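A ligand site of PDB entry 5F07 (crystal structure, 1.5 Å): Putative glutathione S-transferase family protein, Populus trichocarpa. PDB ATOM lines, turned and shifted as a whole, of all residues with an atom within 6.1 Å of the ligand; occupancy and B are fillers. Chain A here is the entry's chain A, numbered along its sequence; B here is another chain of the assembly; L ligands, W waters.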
ATOM      1  N   ALA A  10     -10.647 -26.463 -18.550  1.00  0.00           N
ATOM      2  CA  ALA A  10      -9.927 -26.609 -19.809  1.00  0.00           C
ATOM      3  C   ALA A  10      -9.349 -28.017 -19.969  1.00  0.00           C
ATOM      4  O   ALA A  10      -8.922 -28.641 -19.000  1.00  0.00           O
ATOM      5  CB  ALA A  10      -8.834 -25.591 -19.911  1.00  0.00           C
ATOM      6  N   VAL A  11      -9.348 -28.477 -21.210  1.00  0.00           N
ATOM      7  CA  VAL A  11      -8.915 -29.832 -21.580  1.00  0.00           C
ATOM      8  C   VAL A  11      -7.519 -30.173 -21.079  1.00  0.00           C
ATOM      9  O   VAL A  11      -7.293 -31.234 -20.526  1.00  0.00           O
ATOM     10  CB  VAL A  11      -8.967 -29.987 -23.121  1.00  0.00           C
ATOM     11  CG1 VAL A  11      -8.105 -31.149 -23.657  1.00  0.00           C
ATOM     12  CG2 VAL A  11     -10.410 -30.155 -23.571  1.00  0.00           C
ATOM     13  N   CYS A  12      -6.579 -29.263 -21.312  1.00  0.00           N
ATOM     14  CA  CYS A  12      -5.177 -29.545 -21.061  1.00  0.00           C
ATOM     15  C   CYS A  12      -4.836 -29.656 -19.544  1.00  0.00           C
ATOM     16  O   CYS A  12      -4.213 -30.623 -19.132  1.00  0.00           O
ATOM     17  CB  CYS A  12      -4.317 -28.495 -21.787  1.00  0.00           C
ATOM     18  SG  CYS A  12      -4.843 -28.166 -23.524  1.00  0.00           S
ATOM     19  N   PRO A  13      -5.308 -28.712 -18.708  1.00  0.00           N
ATOM     20  CA  PRO A  13      -5.121 -28.949 -17.264  1.00  0.00           C
ATOM     21  C   PRO A  13      -5.884 -30.158 -16.738  1.00  0.00           C
ATOM     22  O   PRO A  13      -5.404 -30.831 -15.817  1.00  0.00           O
ATOM     23  CB  PRO A  13      -5.664 -27.673 -16.633  1.00  0.00           C
ATOM     24  CG  PRO A  13      -5.482 -26.635 -17.650  1.00  0.00           C
ATOM     25  CD  PRO A  13      -5.780 -27.337 -18.959  1.00  0.00           C
ATOM     26  N   ARG A  15      -6.304 -33.044 -18.147  1.00  0.00           N
ATOM     27  CA  ARG A  15      -5.507 -34.236 -18.354  1.00  0.00           C
ATOM     28  C   ARG A  15      -4.555 -34.452 -17.173  1.00  0.00           C
ATOM     29  O   ARG A  15      -4.429 -35.560 -16.665  1.00  0.00           O
ATOM     30  CB  ARG A  15      -4.743 -34.112 -19.667  1.00  0.00           C
ATOM     31  CG  ARG A  15      -3.981 -35.374 -20.114  1.00  0.00           C
ATOM     32  CD  ARG A  15      -3.343 -35.172 -21.527  1.00  0.00           C
ATOM     33  NE  ARG A  15      -4.374 -34.981 -22.541  1.00  0.00           N
ATOM     34  CZ  ARG A  15      -4.578 -33.879 -23.266  1.00  0.00           C
ATOM     35  NH1 ARG A  15      -3.757 -32.851 -23.185  1.00  0.00           N
ATOM     36  NH2 ARG A  15      -5.591 -33.838 -24.107  1.00  0.00           N
ATOM     37  N   LEU A  34      -7.842 -17.711 -19.308  1.00  0.00           N
ATOM     38  CA  LEU A  34      -7.443 -17.801 -20.709  1.00  0.00           C
ATOM     39  C   LEU A  34      -8.233 -16.848 -21.609  1.00  0.00           C
ATOM     40  O   LEU A  34      -7.700 -16.344 -22.593  1.00  0.00           O
ATOM     41  CB  LEU A  34      -7.599 -19.243 -21.214  1.00  0.00           C
ATOM     42  CG  LEU A  34      -6.806 -20.319 -20.464  1.00  0.00           C
ATOM     43  CD1 LEU A  34      -7.056 -21.698 -21.073  1.00  0.00           C
ATOM     44  CD2 LEU A  34      -5.326 -19.997 -20.412  1.00  0.00           C
ATOM     45  N   GLN A  39      -2.518 -15.877 -19.826  1.00  0.00           N
ATOM     46  CA  GLN A  39      -1.439 -16.806 -20.201  1.00  0.00           C
ATOM     47  C   GLN A  39      -0.391 -16.148 -21.104  1.00  0.00           C
ATOM     48  O   GLN A  39       0.700 -16.684 -21.292  1.00  0.00           O
ATOM     49  CB  GLN A  39      -2.022 -18.056 -20.868  1.00  0.00           C
ATOM     50  CG  GLN A  39      -2.551 -17.852 -22.294  1.00  0.00           C
ATOM     51  CD  GLN A  39      -3.967 -17.274 -22.362  1.00  0.00           C
ATOM     52  OE1 GLN A  39      -4.441 -16.635 -21.425  1.00  0.00           O
ATOM     53  NE2 GLN A  39      -4.647 -17.524 -23.472  1.00  0.00           N
ATOM     54  N   LYS A  40      -0.710 -14.994 -21.676  1.00  0.00           N
ATOM     55  CA  LYS A  40       0.241 -14.295 -22.537  1.00  0.00           C
ATOM     56  C   LYS A  40       0.969 -13.151 -21.808  1.00  0.00           C
ATOM     57  O   LYS A  40       1.817 -12.479 -22.397  1.00  0.00           O
ATOM     58  CB  LYS A  40      -0.462 -13.764 -23.790  1.00  0.00           C
ATOM     59  CG  LYS A  40      -1.198 -14.820 -24.589  1.00  0.00           C
ATOM     60  CD  LYS A  40      -0.296 -15.987 -25.009  1.00  0.00           C
ATOM     61  CE  LYS A  40      -1.062 -17.003 -25.842  1.00  0.00           C
ATOM     62  NZ  LYS A  40      -0.226 -18.186 -26.170  1.00  0.00           N
ATOM     63  N   GLN A  48       5.496 -20.754 -18.308  1.00  0.00           N
ATOM     64  CA  GLN A  48       5.305 -21.527 -19.531  1.00  0.00           C
ATOM     65  C   GLN A  48       5.614 -20.583 -20.700  1.00  0.00           C
ATOM     66  O   GLN A  48       4.828 -19.696 -20.993  1.00  0.00           O
ATOM     67  CB  GLN A  48       3.875 -22.089 -19.611  1.00  0.00           C
ATOM     68  CG  GLN A  48       3.783 -23.518 -20.164  1.00  0.00           C
ATOM     69  CD  GLN A  48       3.889 -23.575 -21.689  1.00  0.00           C
ATOM     70  OE1 GLN A  48       4.457 -22.678 -22.325  1.00  0.00           O
ATOM     71  NE2 GLN A  48       3.328 -24.612 -22.282  1.00  0.00           N
ATOM     72  N   PHE A  50       5.659 -20.659 -23.882  1.00  0.00           N
ATOM     73  CA  PHE A  50       4.783 -20.653 -25.055  1.00  0.00           C
ATOM     74  C   PHE A  50       3.400 -20.075 -24.747  1.00  0.00           C
ATOM     75  O   PHE A  50       2.523 -20.013 -25.606  1.00  0.00           O
ATOM     76  CB  PHE A  50       4.641 -22.078 -25.614  1.00  0.00           C
ATOM     77  CG  PHE A  50       5.914 -22.672 -26.096  1.00  0.00           C
ATOM     78  CD1 PHE A  50       6.415 -22.333 -27.343  1.00  0.00           C
ATOM     79  CD2 PHE A  50       6.629 -23.558 -25.309  1.00  0.00           C
ATOM     80  CE1 PHE A  50       7.591 -22.870 -27.797  1.00  0.00           C
ATOM     81  CE2 PHE A  50       7.803 -24.112 -25.762  1.00  0.00           C
ATOM     82  CZ  PHE A  50       8.300 -23.767 -27.016  1.00  0.00           C
ATOM     83  N   GLY A  51       3.197 -19.633 -23.512  1.00  0.00           N
ATOM     84  CA  GLY A  51       1.962 -18.964 -23.143  1.00  0.00           C
ATOM     85  C   GLY A  51       0.755 -19.888 -23.208  1.00  0.00           C
ATOM     86  O   GLY A  51      -0.311 -19.512 -23.718  1.00  0.00           O
ATOM     87  N   GLN A  52       0.939 -21.093 -22.688  1.00  0.00           N
ATOM     88  CA  GLN A  52      -0.109 -22.108 -22.645  1.00  0.00           C
ATOM     89  C   GLN A  52      -0.133 -22.764 -21.286  1.00  0.00           C
ATOM     90  O   GLN A  52       0.846 -22.699 -20.539  1.00  0.00           O
ATOM     91  CB  GLN A  52       0.104 -23.151 -23.753  1.00  0.00           C
ATOM     92  CG  GLN A  52       0.038 -22.578 -25.148  1.00  0.00           C
ATOM     93  CD  GLN A  52       0.294 -23.589 -26.244  1.00  0.00           C
ATOM     94  OE1 GLN A  52       0.781 -24.694 -26.014  1.00  0.00           O
ATOM     95  NE2 GLN A  52      -0.039 -23.197 -27.458  1.00  0.00           N
ATOM     96  N   VAL A  53      -1.249 -23.427 -20.988  1.00  0.00           N
ATOM     97  CA  VAL A  53      -1.416 -24.202 -19.747  1.00  0.00           C
ATOM     98  C   VAL A  53      -1.657 -25.656 -20.129  1.00  0.00           C
ATOM     99  O   VAL A  53      -2.241 -25.926 -21.175  1.00  0.00           O
ATOM    100  CB  VAL A  53      -2.583 -23.648 -18.871  1.00  0.00           C
ATOM    101  CG1 VAL A  53      -2.278 -22.208 -18.442  1.00  0.00           C
ATOM    102  CG2 VAL A  53      -3.900 -23.719 -19.623  1.00  0.00           C
ATOM    103  N   PRO A  54      -1.266 -26.607 -19.275  1.00  0.00           N
ATOM    104  CA  PRO A  54      -0.765 -26.425 -17.921  1.00  0.00           C
ATOM    105  C   PRO A  54       0.734 -26.314 -17.808  1.00  0.00           C
ATOM    106  O   PRO A  54       1.477 -26.711 -18.700  1.00  0.00           O
ATOM    107  CB  PRO A  54      -1.227 -27.704 -17.220  1.00  0.00           C
ATOM    108  CG  PRO A  54      -1.138 -28.745 -18.299  1.00  0.00           C
ATOM    109  CD  PRO A  54      -1.578 -28.023 -19.561  1.00  0.00           C
ATOM    110  N   PHE A  64       6.286 -28.425 -17.969  1.00  0.00           N
ATOM    111  CA  PHE A  64       5.080 -28.219 -18.774  1.00  0.00           C
ATOM    112  C   PHE A  64       4.980 -29.253 -19.893  1.00  0.00           C
ATOM    113  O   PHE A  64       5.754 -30.219 -19.924  1.00  0.00           O
ATOM    114  CB  PHE A  64       5.002 -26.766 -19.279  1.00  0.00           C
ATOM    115  CG  PHE A  64       6.161 -26.307 -20.145  1.00  0.00           C
ATOM    116  CD1 PHE A  64       7.294 -25.741 -19.575  1.00  0.00           C
ATOM    117  CD2 PHE A  64       6.083 -26.400 -21.528  1.00  0.00           C
ATOM    118  CE1 PHE A  64       8.352 -25.285 -20.373  1.00  0.00           C
ATOM    119  CE2 PHE A  64       7.125 -25.936 -22.323  1.00  0.00           C
ATOM    120  CZ  PHE A  64       8.265 -25.400 -21.753  1.00  0.00           C
ATOM    121  N   GLU A  65       3.954 -29.072 -20.742  1.00  0.00           N
ATOM    122  CA  GLU A  65       3.438 -30.063 -21.713  1.00  0.00           C
ATOM    123  C   GLU A  65       2.685 -31.184 -20.958  1.00  0.00           C
ATOM    124  O   GLU A  65       3.266 -31.989 -20.247  1.00  0.00           O
ATOM    125  CB  GLU A  65       4.537 -30.639 -22.633  1.00  0.00           C
ATOM    126  CG  GLU A  65       4.943 -29.674 -23.735  1.00  0.00           C
ATOM    127  CD  GLU A  65       3.826 -29.411 -24.732  1.00  0.00           C
ATOM    128  OE1 GLU A  65       2.980 -30.303 -24.948  1.00  0.00           O
ATOM    129  OE2 GLU A  65       3.766 -28.296 -25.296  1.00  0.00           O
ATOM    130  N   SER A  66       1.356 -31.204 -21.129  1.00  0.00           N
ATOM    131  CA  SER A  66       0.482 -32.061 -20.335  1.00  0.00           C
ATOM    132  C   SER A  66       0.893 -33.520 -20.377  1.00  0.00           C
ATOM    133  O   SER A  66       0.818 -34.187 -19.346  1.00  0.00           O
ATOM    134  CB  SER A  66      -0.985 -31.949 -20.800  1.00  0.00           C
ATOM    135  OG  SER A  66      -1.139 -32.364 -22.148  1.00  0.00           O
ATOM    136  N   ARG A  67       1.322 -34.022 -21.538  1.00  0.00           N
ATOM    137  CA  ARG A  67       1.630 -35.440 -21.622  1.00  0.00           C
ATOM    138  C   ARG A  67       2.997 -35.777 -21.023  1.00  0.00           C
ATOM    139  O   ARG A  67       3.197 -36.890 -20.570  1.00  0.00           O
ATOM    140  CB  ARG A  67       1.518 -35.918 -23.052  1.00  0.00           C
ATOM    141  CG  ARG A  67       0.088 -35.791 -23.575  1.00  0.00           C
ATOM    142  CD  ARG A  67      -0.047 -36.061 -25.050  1.00  0.00           C
ATOM    143  NE  ARG A  67      -1.361 -35.672 -25.584  1.00  0.00           N
ATOM    144  CZ  ARG A  67      -1.686 -34.429 -25.945  1.00  0.00           C
ATOM    145  NH1 ARG A  67      -0.808 -33.443 -25.820  1.00  0.00           N
ATOM    146  NH2 ARG A  67      -2.885 -34.170 -26.460  1.00  0.00           N
ATOM    147  N   PHE A 111      -9.673 -31.793 -30.814  1.00  0.00           N
ATOM    148  CA  PHE A 111      -9.545 -30.510 -30.156  1.00  0.00           C
ATOM    149  C   PHE A 111      -9.942 -29.405 -31.114  1.00  0.00           C
ATOM    150  O   PHE A 111     -10.500 -28.400 -30.684  1.00  0.00           O
ATOM    151  CB  PHE A 111      -8.125 -30.252 -29.629  1.00  0.00           C
ATOM    152  CG  PHE A 111      -8.020 -28.968 -28.852  1.00  0.00           C
ATOM    153  CD1 PHE A 111      -8.354 -28.930 -27.509  1.00  0.00           C
ATOM    154  CD2 PHE A 111      -7.653 -27.787 -29.494  1.00  0.00           C
ATOM    155  CE1 PHE A 111      -8.299 -27.722 -26.790  1.00  0.00           C
ATOM    156  CE2 PHE A 111      -7.593 -26.592 -28.789  1.00  0.00           C
ATOM    157  CZ  PHE A 111      -7.918 -26.565 -27.433  1.00  0.00           C
ATOM    158  N   GLU B 100       7.709 -33.343 -26.419  1.00  0.00           N
ATOM    159  CA  GLU B 100       6.326 -32.872 -26.615  1.00  0.00           C
ATOM    160  C   GLU B 100       6.281 -31.501 -27.300  1.00  0.00           C
ATOM    161  O   GLU B 100       5.397 -31.217 -28.087  1.00  0.00           O
ATOM    162  CB  GLU B 100       5.584 -32.798 -25.269  1.00  0.00           C
ATOM    163  CG  GLU B 100       5.217 -34.142 -24.629  1.00  0.00           C
ATOM    164  CD  GLU B 100       4.408 -35.026 -25.528  1.00  0.00           C
ATOM    165  OE1 GLU B 100       3.319 -34.607 -26.030  1.00  0.00           O
ATOM    166  OE2 GLU B 100       4.876 -36.178 -25.738  1.00  0.00           O
ATOM    167  N   HIS B 104       4.436 -30.975 -31.160  1.00  0.00           N
ATOM    168  CA  HIS B 104       3.302 -30.090 -31.492  1.00  0.00           C
ATOM    169  C   HIS B 104       3.800 -28.678 -31.886  1.00  0.00           C
ATOM    170  O   HIS B 104       3.774 -28.340 -33.077  1.00  0.00           O
ATOM    171  CB  HIS B 104       2.291 -30.049 -30.342  1.00  0.00           C
ATOM    172  CG  HIS B 104       1.876 -31.416 -29.880  1.00  0.00           C
ATOM    173  ND1 HIS B 104       0.834 -32.108 -30.471  1.00  0.00           N
ATOM    174  CD2 HIS B 104       2.362 -32.226 -28.915  1.00  0.00           C
ATOM    175  CE1 HIS B 104       0.713 -33.286 -29.879  1.00  0.00           C
ATOM    176  NE2 HIS B 104       1.625 -33.379 -28.937  1.00  0.00           N
ATOM    177  N   ASN B 105       4.245 -27.890 -30.917  1.00  0.00           N
ATOM    178  CA  ASN B 105       4.677 -26.496 -31.175  1.00  0.00           C
ATOM    179  C   ASN B 105       5.594 -26.400 -32.398  1.00  0.00           C
ATOM    180  O   ASN B 105       5.368 -25.559 -33.267  1.00  0.00           O
ATOM    181  CB  ASN B 105       5.381 -25.918 -29.942  1.00  0.00           C
ATOM    182  CG  ASN B 105       4.446 -25.713 -28.766  1.00  0.00           C
ATOM    183  OD1 ASN B 105       3.223 -25.780 -28.901  1.00  0.00           O
ATOM    184  ND2 ASN B 105       5.025 -25.490 -27.594  1.00  0.00           N
HETATM  185  N1  LIG L   1       0.775 -29.361 -26.127  1.00  0.00           N
HETATM  186  C1  LIG L   1       0.345 -28.557 -24.979  1.00  0.00           C
HETATM  187  C2  LIG L   1       0.100 -29.473 -23.815  1.00  0.00           C
HETATM  188  O1  LIG L   1       0.271 -29.027 -22.632  1.00  0.00           O
HETATM  189  O2  LIG L   1      -0.322 -30.627 -24.072  1.00  0.00           O
HETATM  190  C3  LIG L   1      -0.957 -27.839 -25.393  1.00  0.00           C
HETATM  191  C4  LIG L   1      -1.414 -26.836 -24.326  1.00  0.00           C
HETATM  192  C5  LIG L   1      -2.599 -26.008 -24.776  1.00  0.00           C
HETATM  193  O3  LIG L   1      -2.946 -25.961 -25.942  1.00  0.00           O
HETATM  194  N2  LIG L   1      -3.203 -25.348 -23.789  1.00  0.00           N
HETATM  195  C6  LIG L   1      -4.433 -24.595 -23.988  1.00  0.00           C
HETATM  196  C7  LIG L   1      -4.188 -23.142 -23.757  1.00  0.00           C
HETATM  197  O4  LIG L   1      -3.358 -22.757 -22.950  1.00  0.00           O
HETATM  198  C8  LIG L   1      -5.497 -25.076 -23.014  1.00  0.00           C
HETATM  199  S1  LIG L   1      -6.280 -26.680 -23.321  1.00  0.00           S
HETATM  200  N3  LIG L   1      -4.943 -22.338 -24.509  1.00  0.00           N
HETATM  201  C9  LIG L   1      -4.757 -20.896 -24.469  1.00  0.00           C
HETATM  202  C10 LIG L   1      -3.794 -20.365 -25.508  1.00  0.00           C
HETATM  203  O5  LIG L   1      -3.573 -19.130 -25.531  1.00  0.00           O
HETATM  204  O6  LIG L   1      -3.245 -21.151 -26.325  1.00  0.00           O
HETATM  205  O   HOH W   1      -1.509 -30.958 -27.555  1.00  0.00           O
HETATM  206  O   HOH W   2       1.821 -27.080 -21.331  1.00  0.00           O
HETATM  207  O   HOH W   3      -7.405 -23.373 -26.025  1.00  0.00           O
HETATM  208  O   HOH W   4      -1.276 -20.335 -27.767  1.00  0.00           O
HETATM  209  O   HOH W   5      -3.734 -18.035 -27.946  1.00  0.00           O
HETATM  210  O   HOH W   6      -8.675 -24.207 -23.725  1.00  0.00           O
HETATM  211  O   HOH W   7      -4.554 -27.686 -27.578  1.00  0.00           O
HETATM  212  O   HOH W   8       1.732 -32.949 -24.310  1.00  0.00           O
HETATM  213  O   HOH W   9      -3.733 -23.656 -27.354  1.00  0.00           O
HETATM  214  O   HOH W  10       1.199 -26.920 -27.766  1.00  0.00           O
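OE1 of Glu 65 lies within salt-bridge range of N1 of the ligand (2.7 Å). NZ of Lys 40 lies within salt-bridge range of O5 of the ligand, at 3.5 Å. N of Cys 12 lies close to S1 of the ligand, at 3.3 Å. S1 of the ligand is bonded to SG of Cys 12 (2.1 Å). The backbone carbonyl oxygen of Val 53 sits at hydrogen-bond distance from a nitrogen (N2) of the ligand (2.8 Å). The side-chain amide nitrogen (NE2) of Gln 39 is in hydrogen-bond range of an oxygen (O5) of the ligand, 2.8 Å away. The backbone NH (N) of Val 53 sits at hydrogen-bond distance from an oxygen (O4) of the ligand (3.0 Å). N of Ser 66 is in hydrogen-bond range of O1 of the ligand, at 2.9 Å. NH1 of Arg 67 lies within salt-bridge range of O2 of the ligand (3.3 Å). An oxygen (O2) of the ligand lies within hydrogen-bond range of the side-chain hydroxyl (OG) of Ser 66 (2.7 Å).
The side-chain amide nitrogen (NE2) of Gln 39 is in hydrogen-bond range of the backbone carbonyl oxygen (O) of Leu 34 (3.4 Å). The side-chain amino group of Lys 40 is in hydrogen-bond range of the backbone carbonyl oxygen of Phe 50 (3.3 Å). O of Gly 51 sits at hydrogen-bond distance from NZ of Lys 40 (2.8 Å). The side-chain hydroxyl (OG) of Ser 66 is in hydrogen-bond range of the guanidinium group (NH1) of Arg 15 (2.9 Å).
O of Gly 51 touches O5 of the ligand (3.8 Å). Gln 52 touches the ligand (CA to O4, 3.3 Å). Pro 54 touches the ligand. Hydrophobic or aromatic side chains within 4 Å of the ligand: Val 53 and Pro 54. Of the 22 residues printed, 10 come within 4 Å of the ligand.
Water W4 lies within hydrogen-bond range of an oxygen (O6) of the ligand (2.6 Å), the side-chain amino group of Lys 40 (2.9 Å) and the side-chain amide nitrogen of Gln 52 (3.1 Å). Water W2 lies within hydrogen-bond range of O of Pro 54 (2.7 Å), O1 of the ligand (2.8 Å), N of Glu 65 (3.0 Å) and NE2 of Gln 48 (3.0 Å). Water W10 lies within hydrogen-bond range of OD1 of Asn 105 of chain B (2.6 Å), OE1 of Gln 52 (2.9 Å) and N1 of the ligand (3.0 Å). Water W8 lies within hydrogen-bond range of the side-chain carboxylate of Glu 100 of chain B (2.9 Å), the side-chain carboxylate of Glu 65 (3.0 Å), the guanidinium group of Arg 67 (3.0 Å) and an oxygen (O2) of the ligand (3.1 Å). Water W1 bridges NH1 of Arg 67 and N1 of the ligand.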
